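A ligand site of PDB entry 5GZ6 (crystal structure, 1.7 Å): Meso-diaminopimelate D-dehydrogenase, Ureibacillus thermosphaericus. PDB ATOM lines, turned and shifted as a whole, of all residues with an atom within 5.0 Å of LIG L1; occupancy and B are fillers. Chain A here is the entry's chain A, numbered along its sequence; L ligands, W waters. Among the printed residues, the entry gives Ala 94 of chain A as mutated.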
ATOM      1  N   VAL A   9      13.085 -28.389  -2.817  1.00  0.00           N
ATOM      2  CA  VAL A   9      12.320 -27.189  -3.119  1.00  0.00           C
ATOM      3  C   VAL A   9      12.179 -26.444  -1.789  1.00  0.00           C
ATOM      4  O   VAL A   9      11.557 -26.947  -0.853  1.00  0.00           O
ATOM      5  CB  VAL A   9      10.925 -27.480  -3.699  1.00  0.00           C
ATOM      6  CG1 VAL A   9      10.109 -26.195  -3.747  1.00  0.00           C
ATOM      7  CG2 VAL A   9      11.050 -28.090  -5.074  1.00  0.00           C
ATOM      8  N   GLY A  10      12.739 -25.247  -1.725  1.00  0.00           N
ATOM      9  CA  GLY A  10      12.705 -24.423  -0.533  1.00  0.00           C
ATOM     10  C   GLY A  10      13.983 -24.635   0.250  1.00  0.00           C
ATOM     11  O   GLY A  10      14.431 -25.765   0.397  1.00  0.00           O
ATOM     12  N   TYR A  11      14.566 -23.565   0.770  1.00  0.00           N
ATOM     13  CA  TYR A  11      15.793 -23.719   1.523  1.00  0.00           C
ATOM     14  C   TYR A  11      15.742 -23.001   2.860  1.00  0.00           C
ATOM     15  O   TYR A  11      16.544 -22.119   3.149  1.00  0.00           O
ATOM     16  CB  TYR A  11      16.986 -23.218   0.698  1.00  0.00           C
ATOM     17  CG  TYR A  11      18.328 -23.695   1.204  1.00  0.00           C
ATOM     18  CD1 TYR A  11      18.701 -25.028   1.122  1.00  0.00           C
ATOM     19  CD2 TYR A  11      19.236 -22.796   1.747  1.00  0.00           C
ATOM     20  CE1 TYR A  11      19.931 -25.458   1.579  1.00  0.00           C
ATOM     21  CE2 TYR A  11      20.474 -23.215   2.207  1.00  0.00           C
ATOM     22  CZ  TYR A  11      20.811 -24.546   2.121  1.00  0.00           C
ATOM     23  OH  TYR A  11      22.036 -24.964   2.582  1.00  0.00           O
ATOM     24  N   GLY A  12      14.799 -23.431   3.678  1.00  0.00           N
ATOM     25  CA  GLY A  12      14.607 -22.944   5.020  1.00  0.00           C
ATOM     26  C   GLY A  12      15.380 -23.924   5.877  1.00  0.00           C
ATOM     27  O   GLY A  12      16.084 -24.778   5.343  1.00  0.00           O
ATOM     28  N   ASN A  13      15.206 -23.876   7.189  1.00  0.00           N
ATOM     29  CA  ASN A  13      15.956 -24.792   8.042  1.00  0.00           C
ATOM     30  C   ASN A  13      15.680 -26.239   7.649  1.00  0.00           C
ATOM     31  O   ASN A  13      16.583 -27.072   7.673  1.00  0.00           O
ATOM     32  CB  ASN A  13      15.697 -24.536   9.524  1.00  0.00           C
ATOM     33  CG  ASN A  13      14.223 -24.601   9.883  1.00  0.00           C
ATOM     34  OD1 ASN A  13      13.560 -25.606   9.643  1.00  0.00           O
ATOM     35  ND2 ASN A  13      13.713 -23.531  10.478  1.00  0.00           N
ATOM     36  N   LEU A  14      14.441 -26.543   7.282  1.00  0.00           N
ATOM     37  CA  LEU A  14      14.116 -27.895   6.847  1.00  0.00           C
ATOM     38  C   LEU A  14      14.868 -28.272   5.570  1.00  0.00           C
ATOM     39  O   LEU A  14      15.378 -29.384   5.456  1.00  0.00           O
ATOM     40  CB  LEU A  14      12.609 -28.015   6.627  1.00  0.00           C
ATOM     41  CG  LEU A  14      12.092 -29.429   6.415  1.00  0.00           C
ATOM     42  CD1 LEU A  14      12.386 -30.274   7.647  1.00  0.00           C
ATOM     43  CD2 LEU A  14      10.600 -29.399   6.141  1.00  0.00           C
ATOM     44  N   GLY A  15      14.954 -27.341   4.620  1.00  0.00           N
ATOM     45  CA  GLY A  15      15.651 -27.588   3.365  1.00  0.00           C
ATOM     46  C   GLY A  15      17.124 -27.841   3.636  1.00  0.00           C
ATOM     47  O   GLY A  15      17.735 -28.741   3.068  1.00  0.00           O
ATOM     48  N   PHE A  34      15.906 -25.515  -5.287  1.00  0.00           N
ATOM     49  CA  PHE A  34      15.028 -24.533  -5.930  1.00  0.00           C
ATOM     50  C   PHE A  34      14.530 -23.560  -4.888  1.00  0.00           C
ATOM     51  O   PHE A  34      14.086 -23.965  -3.810  1.00  0.00           O
ATOM     52  CB  PHE A  34      13.875 -25.228  -6.652  1.00  0.00           C
ATOM     53  CG  PHE A  34      14.332 -26.159  -7.734  1.00  0.00           C
ATOM     54  CD1 PHE A  34      14.561 -25.698  -9.011  1.00  0.00           C
ATOM     55  CD2 PHE A  34      14.564 -27.500  -7.459  1.00  0.00           C
ATOM     56  CE1 PHE A  34      14.991 -26.554 -10.010  1.00  0.00           C
ATOM     57  CE2 PHE A  34      14.987 -28.353  -8.452  1.00  0.00           C
ATOM     58  CZ  PHE A  34      15.203 -27.881  -9.731  1.00  0.00           C
ATOM     59  N   THR A  35      14.619 -22.266  -5.182  1.00  0.00           N
ATOM     60  CA  THR A  35      14.240 -21.281  -4.195  1.00  0.00           C
ATOM     61  C   THR A  35      13.490 -20.131  -4.813  1.00  0.00           C
ATOM     62  O   THR A  35      13.632 -19.851  -6.017  1.00  0.00           O
ATOM     63  CB  THR A  35      15.518 -20.748  -3.446  1.00  0.00           C
ATOM     64  OG1 THR A  35      15.176 -19.909  -2.292  1.00  0.00           O
ATOM     65  CG2 THR A  35      16.442 -20.076  -4.428  1.00  0.00           C
ATOM     66  N   ARG A  36      12.649 -19.508  -4.003  1.00  0.00           N
ATOM     67  CA  ARG A  36      11.929 -18.288  -4.415  1.00  0.00           C
ATOM     68  C   ARG A  36      12.822 -17.087  -4.284  1.00  0.00           C
ATOM     69  O   ARG A  36      12.522 -16.083  -4.863  1.00  0.00           O
ATOM     70  CB  ARG A  36      10.722 -17.974  -3.525  1.00  0.00           C
ATOM     71  CG  ARG A  36       9.702 -19.131  -3.507  1.00  0.00           C
ATOM     72  CD  ARG A  36       8.401 -18.928  -2.651  1.00  0.00           C
ATOM     73  NE  ARG A  36       7.413 -19.917  -3.169  1.00  0.00           N
ATOM     74  CZ  ARG A  36       6.193 -20.207  -2.685  1.00  0.00           C
ATOM     75  NH1 ARG A  36       5.704 -19.602  -1.599  1.00  0.00           N
ATOM     76  NH2 ARG A  36       5.426 -21.130  -3.318  1.00  0.00           N
ATOM     77  N   ARG A  37      13.872 -17.187  -3.485  1.00  0.00           N
ATOM     78  CA  ARG A  37      14.794 -16.082  -3.286  1.00  0.00           C
ATOM     79  C   ARG A  37      15.802 -15.997  -4.428  1.00  0.00           C
ATOM     80  O   ARG A  37      15.973 -16.952  -5.176  1.00  0.00           O
ATOM     81  CB  ARG A  37      15.526 -16.230  -1.960  1.00  0.00           C
ATOM     82  CG  ARG A  37      14.617 -16.117  -0.748  1.00  0.00           C
ATOM     83  CD  ARG A  37      15.400 -16.349   0.534  1.00  0.00           C
ATOM     84  NE  ARG A  37      14.520 -16.617   1.672  1.00  0.00           N
ATOM     85  CZ  ARG A  37      13.901 -15.686   2.388  1.00  0.00           C
ATOM     86  NH1 ARG A  37      14.045 -14.403   2.077  1.00  0.00           N
ATOM     87  NH2 ARG A  37      13.139 -16.032   3.398  1.00  0.00           N
ATOM     88  N   VAL A  42      21.616 -17.185  -1.738  1.00  0.00           N
ATOM     89  CA  VAL A  42      21.297 -18.372  -0.936  1.00  0.00           C
ATOM     90  C   VAL A  42      22.548 -19.159  -0.696  1.00  0.00           C
ATOM     91  O   VAL A  42      23.158 -19.544  -1.645  1.00  0.00           O
ATOM     92  CB  VAL A  42      20.230 -19.176  -1.675  1.00  0.00           C
ATOM     93  CG1 VAL A  42      19.949 -20.441  -0.904  1.00  0.00           C
ATOM     94  CG2 VAL A  42      18.951 -18.350  -1.663  1.00  0.00           C
ATOM     95  N   CYS A  69      10.320 -28.761   1.057  1.00  0.00           N
ATOM     96  CA  CYS A  69      10.624 -28.308   2.402  1.00  0.00           C
ATOM     97  C   CYS A  69       9.913 -27.010   2.805  1.00  0.00           C
ATOM     98  O   CYS A  69      10.271 -26.380   3.796  1.00  0.00           O
ATOM     99  CB  CYS A  69      12.132 -28.214   2.579  1.00  0.00           C
ATOM    100  SG  CYS A  69      12.975 -29.725   2.062  1.00  0.00           S
ATOM    101  N   GLY A  70       8.926 -26.624   2.020  1.00  0.00           N
ATOM    102  CA  GLY A  70       8.158 -25.418   2.272  1.00  0.00           C
ATOM    103  C   GLY A  70       7.209 -25.513   3.457  1.00  0.00           C
ATOM    104  O   GLY A  70       6.898 -26.610   3.917  1.00  0.00           O
ATOM    105  N   GLY A  71       6.757 -24.369   3.945  1.00  0.00           N
ATOM    106  CA  GLY A  71       5.836 -24.303   5.055  1.00  0.00           C
ATOM    107  C   GLY A  71       4.440 -24.790   4.701  1.00  0.00           C
ATOM    108  O   GLY A  71       3.971 -24.601   3.588  1.00  0.00           O
ATOM    109  N   SER A  72       3.797 -25.430   5.665  1.00  0.00           N
ATOM    110  CA  SER A  72       2.451 -25.966   5.488  1.00  0.00           C
ATOM    111  C   SER A  72       1.356 -24.931   5.234  1.00  0.00           C
ATOM    112  O   SER A  72       0.447 -25.159   4.451  1.00  0.00           O
ATOM    113  CB  SER A  72       2.065 -26.859   6.676  1.00  0.00           C
ATOM    114  OG  SER A  72       3.012 -27.886   6.853  1.00  0.00           O
ATOM    115  N   ALA A  73       1.423 -23.812   5.937  1.00  0.00           N
ATOM    116  CA  ALA A  73       0.400 -22.783   5.805  1.00  0.00           C
ATOM    117  C   ALA A  73       0.269 -22.112   4.428  1.00  0.00           C
ATOM    118  O   ALA A  73      -0.848 -21.964   3.928  1.00  0.00           O
ATOM    119  CB  ALA A  73       0.586 -21.715   6.874  1.00  0.00           C
ATOM    120  N   ASP A  75       3.189 -22.322   1.619  1.00  0.00           N
ATOM    121  CA  ASP A  75       4.014 -22.907   0.526  1.00  0.00           C
ATOM    122  C   ASP A  75       3.370 -24.181  -0.013  1.00  0.00           C
ATOM    123  O   ASP A  75       3.081 -24.264  -1.157  1.00  0.00           O
ATOM    124  CB  ASP A  75       5.409 -23.157   0.993  1.00  0.00           C
ATOM    125  CG  ASP A  75       6.122 -21.913   1.438  1.00  0.00           C
ATOM    126  OD1 ASP A  75       5.797 -20.818   0.868  1.00  0.00           O
ATOM    127  OD2 ASP A  75       7.056 -22.115   2.278  1.00  0.00           O
ATOM    128  N   SER A  92       6.193 -32.606   4.348  1.00  0.00           N
ATOM    129  CA  SER A  92       5.877 -32.730   5.765  1.00  0.00           C
ATOM    130  C   SER A  92       4.637 -31.907   6.136  1.00  0.00           C
ATOM    131  O   SER A  92       4.573 -31.333   7.216  1.00  0.00           O
ATOM    132  CB  SER A  92       7.066 -32.291   6.618  1.00  0.00           C
ATOM    133  OG  SER A  92       7.331 -30.908   6.439  1.00  0.00           O
ATOM    134  N   ALA A  94       1.704 -30.273   7.677  1.00  0.00           N
ATOM    135  CA  ALA A  94       1.430 -30.567   9.051  1.00  0.00           C
ATOM    136  C   ALA A  94       0.119 -30.003   9.572  1.00  0.00           C
ATOM    137  O   ALA A  94      -0.119 -30.120  10.760  1.00  0.00           O
ATOM    138  CB  ALA A  94       2.532 -30.062   9.882  1.00  0.00           C
ATOM    139  N   SER A 120       2.875 -35.486   4.406  1.00  0.00           N
ATOM    140  CA  SER A 120       2.760 -35.459   5.794  1.00  0.00           C
ATOM    141  C   SER A 120       3.746 -36.429   6.526  1.00  0.00           C
ATOM    142  O   SER A 120       3.349 -37.110   7.499  1.00  0.00           O
ATOM    143  CB  SER A 120       1.320 -35.732   6.176  1.00  0.00           C
ATOM    144  OG  SER A 120       0.487 -34.765   5.593  1.00  0.00           O
ATOM    145  N   VAL A 121       4.993 -36.427   6.079  1.00  0.00           N
ATOM    146  CA  VAL A 121       6.059 -37.227   6.653  1.00  0.00           C
ATOM    147  C   VAL A 121       6.760 -36.395   7.731  1.00  0.00           C
ATOM    148  O   VAL A 121       6.935 -35.186   7.578  1.00  0.00           O
ATOM    149  CB  VAL A 121       7.076 -37.659   5.592  1.00  0.00           C
ATOM    150  CG1 VAL A 121       8.311 -38.279   6.235  1.00  0.00           C
ATOM    151  CG2 VAL A 121       6.430 -38.623   4.606  1.00  0.00           C
ATOM    152  N   GLY A 122       7.153 -37.043   8.824  1.00  0.00           N
ATOM    153  CA  GLY A 122       7.823 -36.349   9.893  1.00  0.00           C
ATOM    154  C   GLY A 122       7.480 -36.917  11.258  1.00  0.00           C
ATOM    155  O   GLY A 122       6.916 -38.003  11.351  1.00  0.00           O
ATOM    156  N   TRP A 123       7.851 -36.202  12.308  1.00  0.00           N
ATOM    157  CA  TRP A 123       7.559 -36.631  13.656  1.00  0.00           C
ATOM    158  C   TRP A 123       6.048 -36.616  13.961  1.00  0.00           C
ATOM    159  O   TRP A 123       5.509 -37.605  14.454  1.00  0.00           O
ATOM    160  CB  TRP A 123       8.360 -35.735  14.611  1.00  0.00           C
ATOM    161  CG  TRP A 123       7.913 -35.685  16.005  1.00  0.00           C
ATOM    162  CD1 TRP A 123       7.146 -36.592  16.668  1.00  0.00           C
ATOM    163  CD2 TRP A 123       8.250 -34.661  16.959  1.00  0.00           C
ATOM    164  NE1 TRP A 123       6.969 -36.197  17.966  1.00  0.00           N
ATOM    165  CE2 TRP A 123       7.637 -35.012  18.173  1.00  0.00           C
ATOM    166  CE3 TRP A 123       9.004 -33.494  16.899  1.00  0.00           C
ATOM    167  CZ2 TRP A 123       7.744 -34.231  19.312  1.00  0.00           C
ATOM    168  CZ3 TRP A 123       9.110 -32.717  18.025  1.00  0.00           C
ATOM    169  CH2 TRP A 123       8.492 -33.097  19.219  1.00  0.00           C
ATOM    170  N   ASP A 124       5.384 -35.519  13.638  1.00  0.00           N
ATOM    171  CA  ASP A 124       3.931 -35.416  13.816  1.00  0.00           C
ATOM    172  C   ASP A 124       3.389 -34.292  12.943  1.00  0.00           C
ATOM    173  O   ASP A 124       3.619 -33.127  13.250  1.00  0.00           O
ATOM    174  CB  ASP A 124       3.523 -35.200  15.268  1.00  0.00           C
ATOM    175  CG  ASP A 124       2.030 -35.399  15.488  1.00  0.00           C
ATOM    176  OD1 ASP A 124       1.313 -35.693  14.510  1.00  0.00           O
ATOM    177  OD2 ASP A 124       1.568 -35.274  16.639  1.00  0.00           O
ATOM    178  N   PRO A 125       2.672 -34.598  11.872  1.00  0.00           N
ATOM    179  CA  PRO A 125       2.342 -35.909  11.400  1.00  0.00           C
ATOM    180  C   PRO A 125       3.552 -36.762  11.059  1.00  0.00           C
ATOM    181  O   PRO A 125       4.644 -36.276  10.852  1.00  0.00           O
ATOM    182  CB  PRO A 125       1.631 -35.666  10.108  1.00  0.00           C
ATOM    183  CG  PRO A 125       1.424 -34.253   9.978  1.00  0.00           C
ATOM    184  CD  PRO A 125       2.316 -33.534  10.909  1.00  0.00           C
ATOM    185  N   SER A 153       9.914 -21.895  16.389  1.00  0.00           N
ATOM    186  CA  SER A 153      10.490 -21.138  15.287  1.00  0.00           C
ATOM    187  C   SER A 153      10.372 -19.647  15.580  1.00  0.00           C
ATOM    188  O   SER A 153      11.002 -18.819  14.929  1.00  0.00           O
ATOM    189  CB  SER A 153       9.801 -21.475  13.960  1.00  0.00           C
ATOM    190  OG  SER A 153      10.088 -22.805  13.563  1.00  0.00           O
ATOM    191  N   THR A 280      12.792 -34.815  11.121  1.00  0.00           N
ATOM    192  CA  THR A 280      11.941 -34.630   9.955  1.00  0.00           C
ATOM    193  C   THR A 280      12.730 -34.552   8.651  1.00  0.00           C
ATOM    194  O   THR A 280      12.320 -35.138   7.651  1.00  0.00           O
ATOM    195  CB  THR A 280      11.016 -33.422  10.112  1.00  0.00           C
ATOM    196  OG1 THR A 280      10.223 -33.587  11.295  1.00  0.00           O
ATOM    197  CG2 THR A 280      10.090 -33.299   8.906  1.00  0.00           C
HETATM  198  P1  LIG L   1      10.740 -22.408   7.301  1.00  0.00           P
HETATM  199  O1  LIG L   1       9.919 -21.172   7.565  1.00  0.00           O
HETATM  200  O2  LIG L   1      12.127 -22.489   7.883  1.00  0.00           O
HETATM  201  O3  LIG L   1      10.846 -22.625   5.709  1.00  0.00           O
HETATM  202  C1  LIG L   1       9.695 -22.573   4.870  1.00  0.00           C
HETATM  203  C2  LIG L   1       9.962 -21.831   3.559  1.00  0.00           C
HETATM  204  O4  LIG L   1      10.399 -20.493   3.776  1.00  0.00           O
HETATM  205  C3  LIG L   1      10.999 -22.499   2.675  1.00  0.00           C
HETATM  206  O5  LIG L   1      10.355 -23.229   1.630  1.00  0.00           O
HETATM  207  C4  LIG L   1      11.840 -21.377   2.095  1.00  0.00           C
HETATM  208  O6  LIG L   1      11.541 -21.161   0.713  1.00  0.00           O
HETATM  209  C5  LIG L   1      11.502 -20.148   2.939  1.00  0.00           C
HETATM  210  N1  LIG L   1      12.665 -19.865   3.796  1.00  0.00           N
HETATM  211  C6  LIG L   1      12.663 -19.831   5.140  1.00  0.00           C
HETATM  212  N2  LIG L   1      13.901 -19.548   5.627  1.00  0.00           N
HETATM  213  C7  LIG L   1      14.709 -19.393   4.573  1.00  0.00           C
HETATM  214  C8  LIG L   1      16.137 -19.079   4.359  1.00  0.00           C
HETATM  215  N3  LIG L   1      16.963 -18.874   5.415  1.00  0.00           N
HETATM  216  N4  LIG L   1      16.592 -19.011   3.088  1.00  0.00           N
HETATM  217  C9  LIG L   1      15.788 -19.217   2.036  1.00  0.00           C
HETATM  218  N5  LIG L   1      14.478 -19.494   2.142  1.00  0.00           N
HETATM  219  C10 LIG L   1      13.893 -19.602   3.358  1.00  0.00           C
HETATM  220  O7  LIG L   1       9.903 -23.687   7.801  1.00  0.00           O
HETATM  221  P2  LIG L   1      10.610 -25.101   8.146  1.00  0.00           P
HETATM  222  O8  LIG L   1      11.164 -25.045   9.548  1.00  0.00           O
HETATM  223  O9  LIG L   1      11.535 -25.422   7.011  1.00  0.00           O
HETATM  224  O10 LIG L   1       9.368 -26.130   8.136  1.00  0.00           O
HETATM  225  C11 LIG L   1       8.472 -26.175   7.032  1.00  0.00           C
HETATM  226  C12 LIG L   1       7.140 -26.836   7.371  1.00  0.00           C
HETATM  227  O11 LIG L   1       7.278 -28.233   7.615  1.00  0.00           O
HETATM  228  C13 LIG L   1       6.469 -26.236   8.607  1.00  0.00           C
HETATM  229  O12 LIG L   1       5.401 -25.381   8.217  1.00  0.00           O
HETATM  230  C14 LIG L   1       5.934 -27.421   9.386  1.00  0.00           C
HETATM  231  O13 LIG L   1       4.507 -27.358   9.492  1.00  0.00           O
HETATM  232  C15 LIG L   1       6.319 -28.656   8.598  1.00  0.00           C
HETATM  233  N6  LIG L   1       6.934 -29.605   9.500  1.00  0.00           N
HETATM  234  C16 LIG L   1       6.349 -30.782   9.755  1.00  0.00           C
HETATM  235  C17 LIG L   1       6.937 -31.691  10.616  1.00  0.00           C
HETATM  236  C18 LIG L   1       6.316 -33.022  10.906  1.00  0.00           C
HETATM  237  O14 LIG L   1       5.594 -33.571  10.078  1.00  0.00           O
HETATM  238  N7  LIG L   1       6.605 -33.565  12.086  1.00  0.00           N
HETATM  239  C19 LIG L   1       8.249 -31.392  11.315  1.00  0.00           C
HETATM  240  C20 LIG L   1       8.763 -30.086  10.955  1.00  0.00           C
HETATM  241  C21 LIG L   1       8.093 -29.253  10.070  1.00  0.00           C
HETATM  242  P3  LIG L   1      12.548 -20.436  -0.305  1.00  0.00           P
HETATM  243  O15 LIG L   1      11.841 -20.571  -1.610  1.00  0.00           O
HETATM  244  O16 LIG L   1      12.656 -19.035   0.212  1.00  0.00           O
HETATM  245  O17 LIG L   1      13.852 -21.154  -0.245  1.00  0.00           O
HETATM  246  O1  LG2 L   2       9.782 -27.978  14.641  1.00  0.00           O
HETATM  247  C1  LG2 L   2       9.255 -29.126  14.752  1.00  0.00           C
HETATM  248  O2  LG2 L   2       9.883 -30.097  15.268  1.00  0.00           O
HETATM  249  C2  LG2 L   2       7.873 -29.378  14.195  1.00  0.00           C
HETATM  250  O3  LG2 L   2       7.200 -28.458  13.731  1.00  0.00           O
HETATM  251  C3  LG2 L   2       7.282 -30.824  14.409  1.00  0.00           C
HETATM  252  C4  LG2 L   2       6.490 -30.711  15.653  1.00  0.00           C
HETATM  253  C5  LG2 L   2       5.686 -31.921  15.787  1.00  0.00           C
HETATM  254  C6  LG2 L   2       4.986 -31.716  17.072  1.00  0.00           C
HETATM  255  N1  LG2 L   2       3.944 -30.668  16.929  1.00  0.00           N
HETATM  256  O   HOH W   1      10.131 -26.989  11.624  1.00  0.00           O
HETATM  257  O   HOH W   2       7.279 -26.459  12.305  1.00  0.00           O
HETATM  258  O   HOH W   3      12.930 -25.217   4.249  1.00  0.00           O
HETATM  259  O   HOH W   4      11.192 -17.061   1.058  1.00  0.00           O
HETATM  260  O   HOH W   5       4.550 -30.519  12.377  1.00  0.00           O
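An oxygen (O2) of LIG L1 sits at hydrogen-bond distance from the backbone NH (N) of Asn 13 (3.4 Å). An oxygen (O8) of LIG L1 sits close to the side-chain amide oxygen (OD1) of Asn 13 (2.5 Å). N of Tyr 11 lies within hydrogen-bond range of O17 of LIG L1 (2.7 Å). The side-chain hydroxyl (OG1) of Thr 35 lies within hydrogen-bond range of an oxygen (O17) of LIG L1, 2.7 Å away. An oxygen (O15) of LIG L1 is in hydrogen-bond range of the backbone NH (N) of Arg 36 (2.7 Å). The backbone carbonyl oxygen (O) of Asp 124 lies within hydrogen-bond range of a nitrogen (N7) of LIG L1, at 3.2 Å. N of Leu 14 sits close to O9 of LIG L1 (3.1 Å). An oxygen (O16) of LIG L1 is in salt-bridge range of the guanidinium group (NE) of Arg 37. OG of Ser 92 sits at hydrogen-bond distance from O11 of LIG L1 (2.9 Å). N of Ser 72 is in hydrogen-bond range of O12 of LIG L1 (3.0 Å). The side-chain hydroxyl of Ser 72 sits at hydrogen-bond distance from an oxygen (O13) of LIG L1.
OG1 of Thr 35 lies within hydrogen-bond range of N of Arg 37 (3.2 Å). OD1 of Asp 75 lies within salt-bridge range of NH1 of Arg 36, at 2.8 Å. N of Ala 94 is in hydrogen-bond range of OG of Ser 72 (2.8 Å). OD2 of Asp 75 is in hydrogen-bond range of N of Gly 71. N of Gly 10 sits at hydrogen-bond distance from O of Phe 34 (2.8 Å). The backbone NH (N) of Cys 69 is in hydrogen-bond range of the backbone carbonyl oxygen (O) of Val 9, at 2.9 Å.
The backbone carbonyl oxygen of Val 121 sits close to an oxygen (O14) of LIG L1, at 3.3 Å. A nitrogen (N7) of LIG L1 lies close to the backbone NH of Trp 123, at 2.9 Å. O of Pro 125 sits close to O14 of LIG L1, at 3.0 Å. Merely in contact with LIG L1: Gly 10 (3.4 Å), Gly 12 (3.5 Å), Cys 69 (3.6 Å), Gly 70 (3.2 Å), Gly 71 (3.4 Å), Asp 75 (3.2 Å), Ala 94 (3.4 Å), Gly 122 (3.6 Å) and Thr 280 (3.0 Å). Hydrophobic or aromatic side chains that line LIG L1: Tyr 11, Leu 14, Ala 94, Trp 123 and Pro 125. 21 residues have an atom within 4 Å of LIG L1: Gly 10, Tyr 11, Gly 12, Asn 13, Leu 14, Thr 35, Arg 36, Arg 37, Cys 69, Gly 70, Gly 71, Ser 72, Asp 75, Ser 92, Ala 94, Val 121, Gly 122, Trp 123, Asp 124, Pro 125 and Thr 280.
Water W4 lies within hydrogen-bond range of O16 of LIG L1 (2.6 Å) and NH2 of Arg 37 (3.2 Å). Water W1 lies within hydrogen-bond range of an oxygen (O8) of LIG L1 and an oxygen (O1) of LG2 L2. Water W3 lies within hydrogen-bond range of the backbone NH (N) of Gly 12, the backbone carbonyl oxygen (O) of Cys 69, the backbone NH (N) of Gly 15 and an oxygen (O9) of LIG L1.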
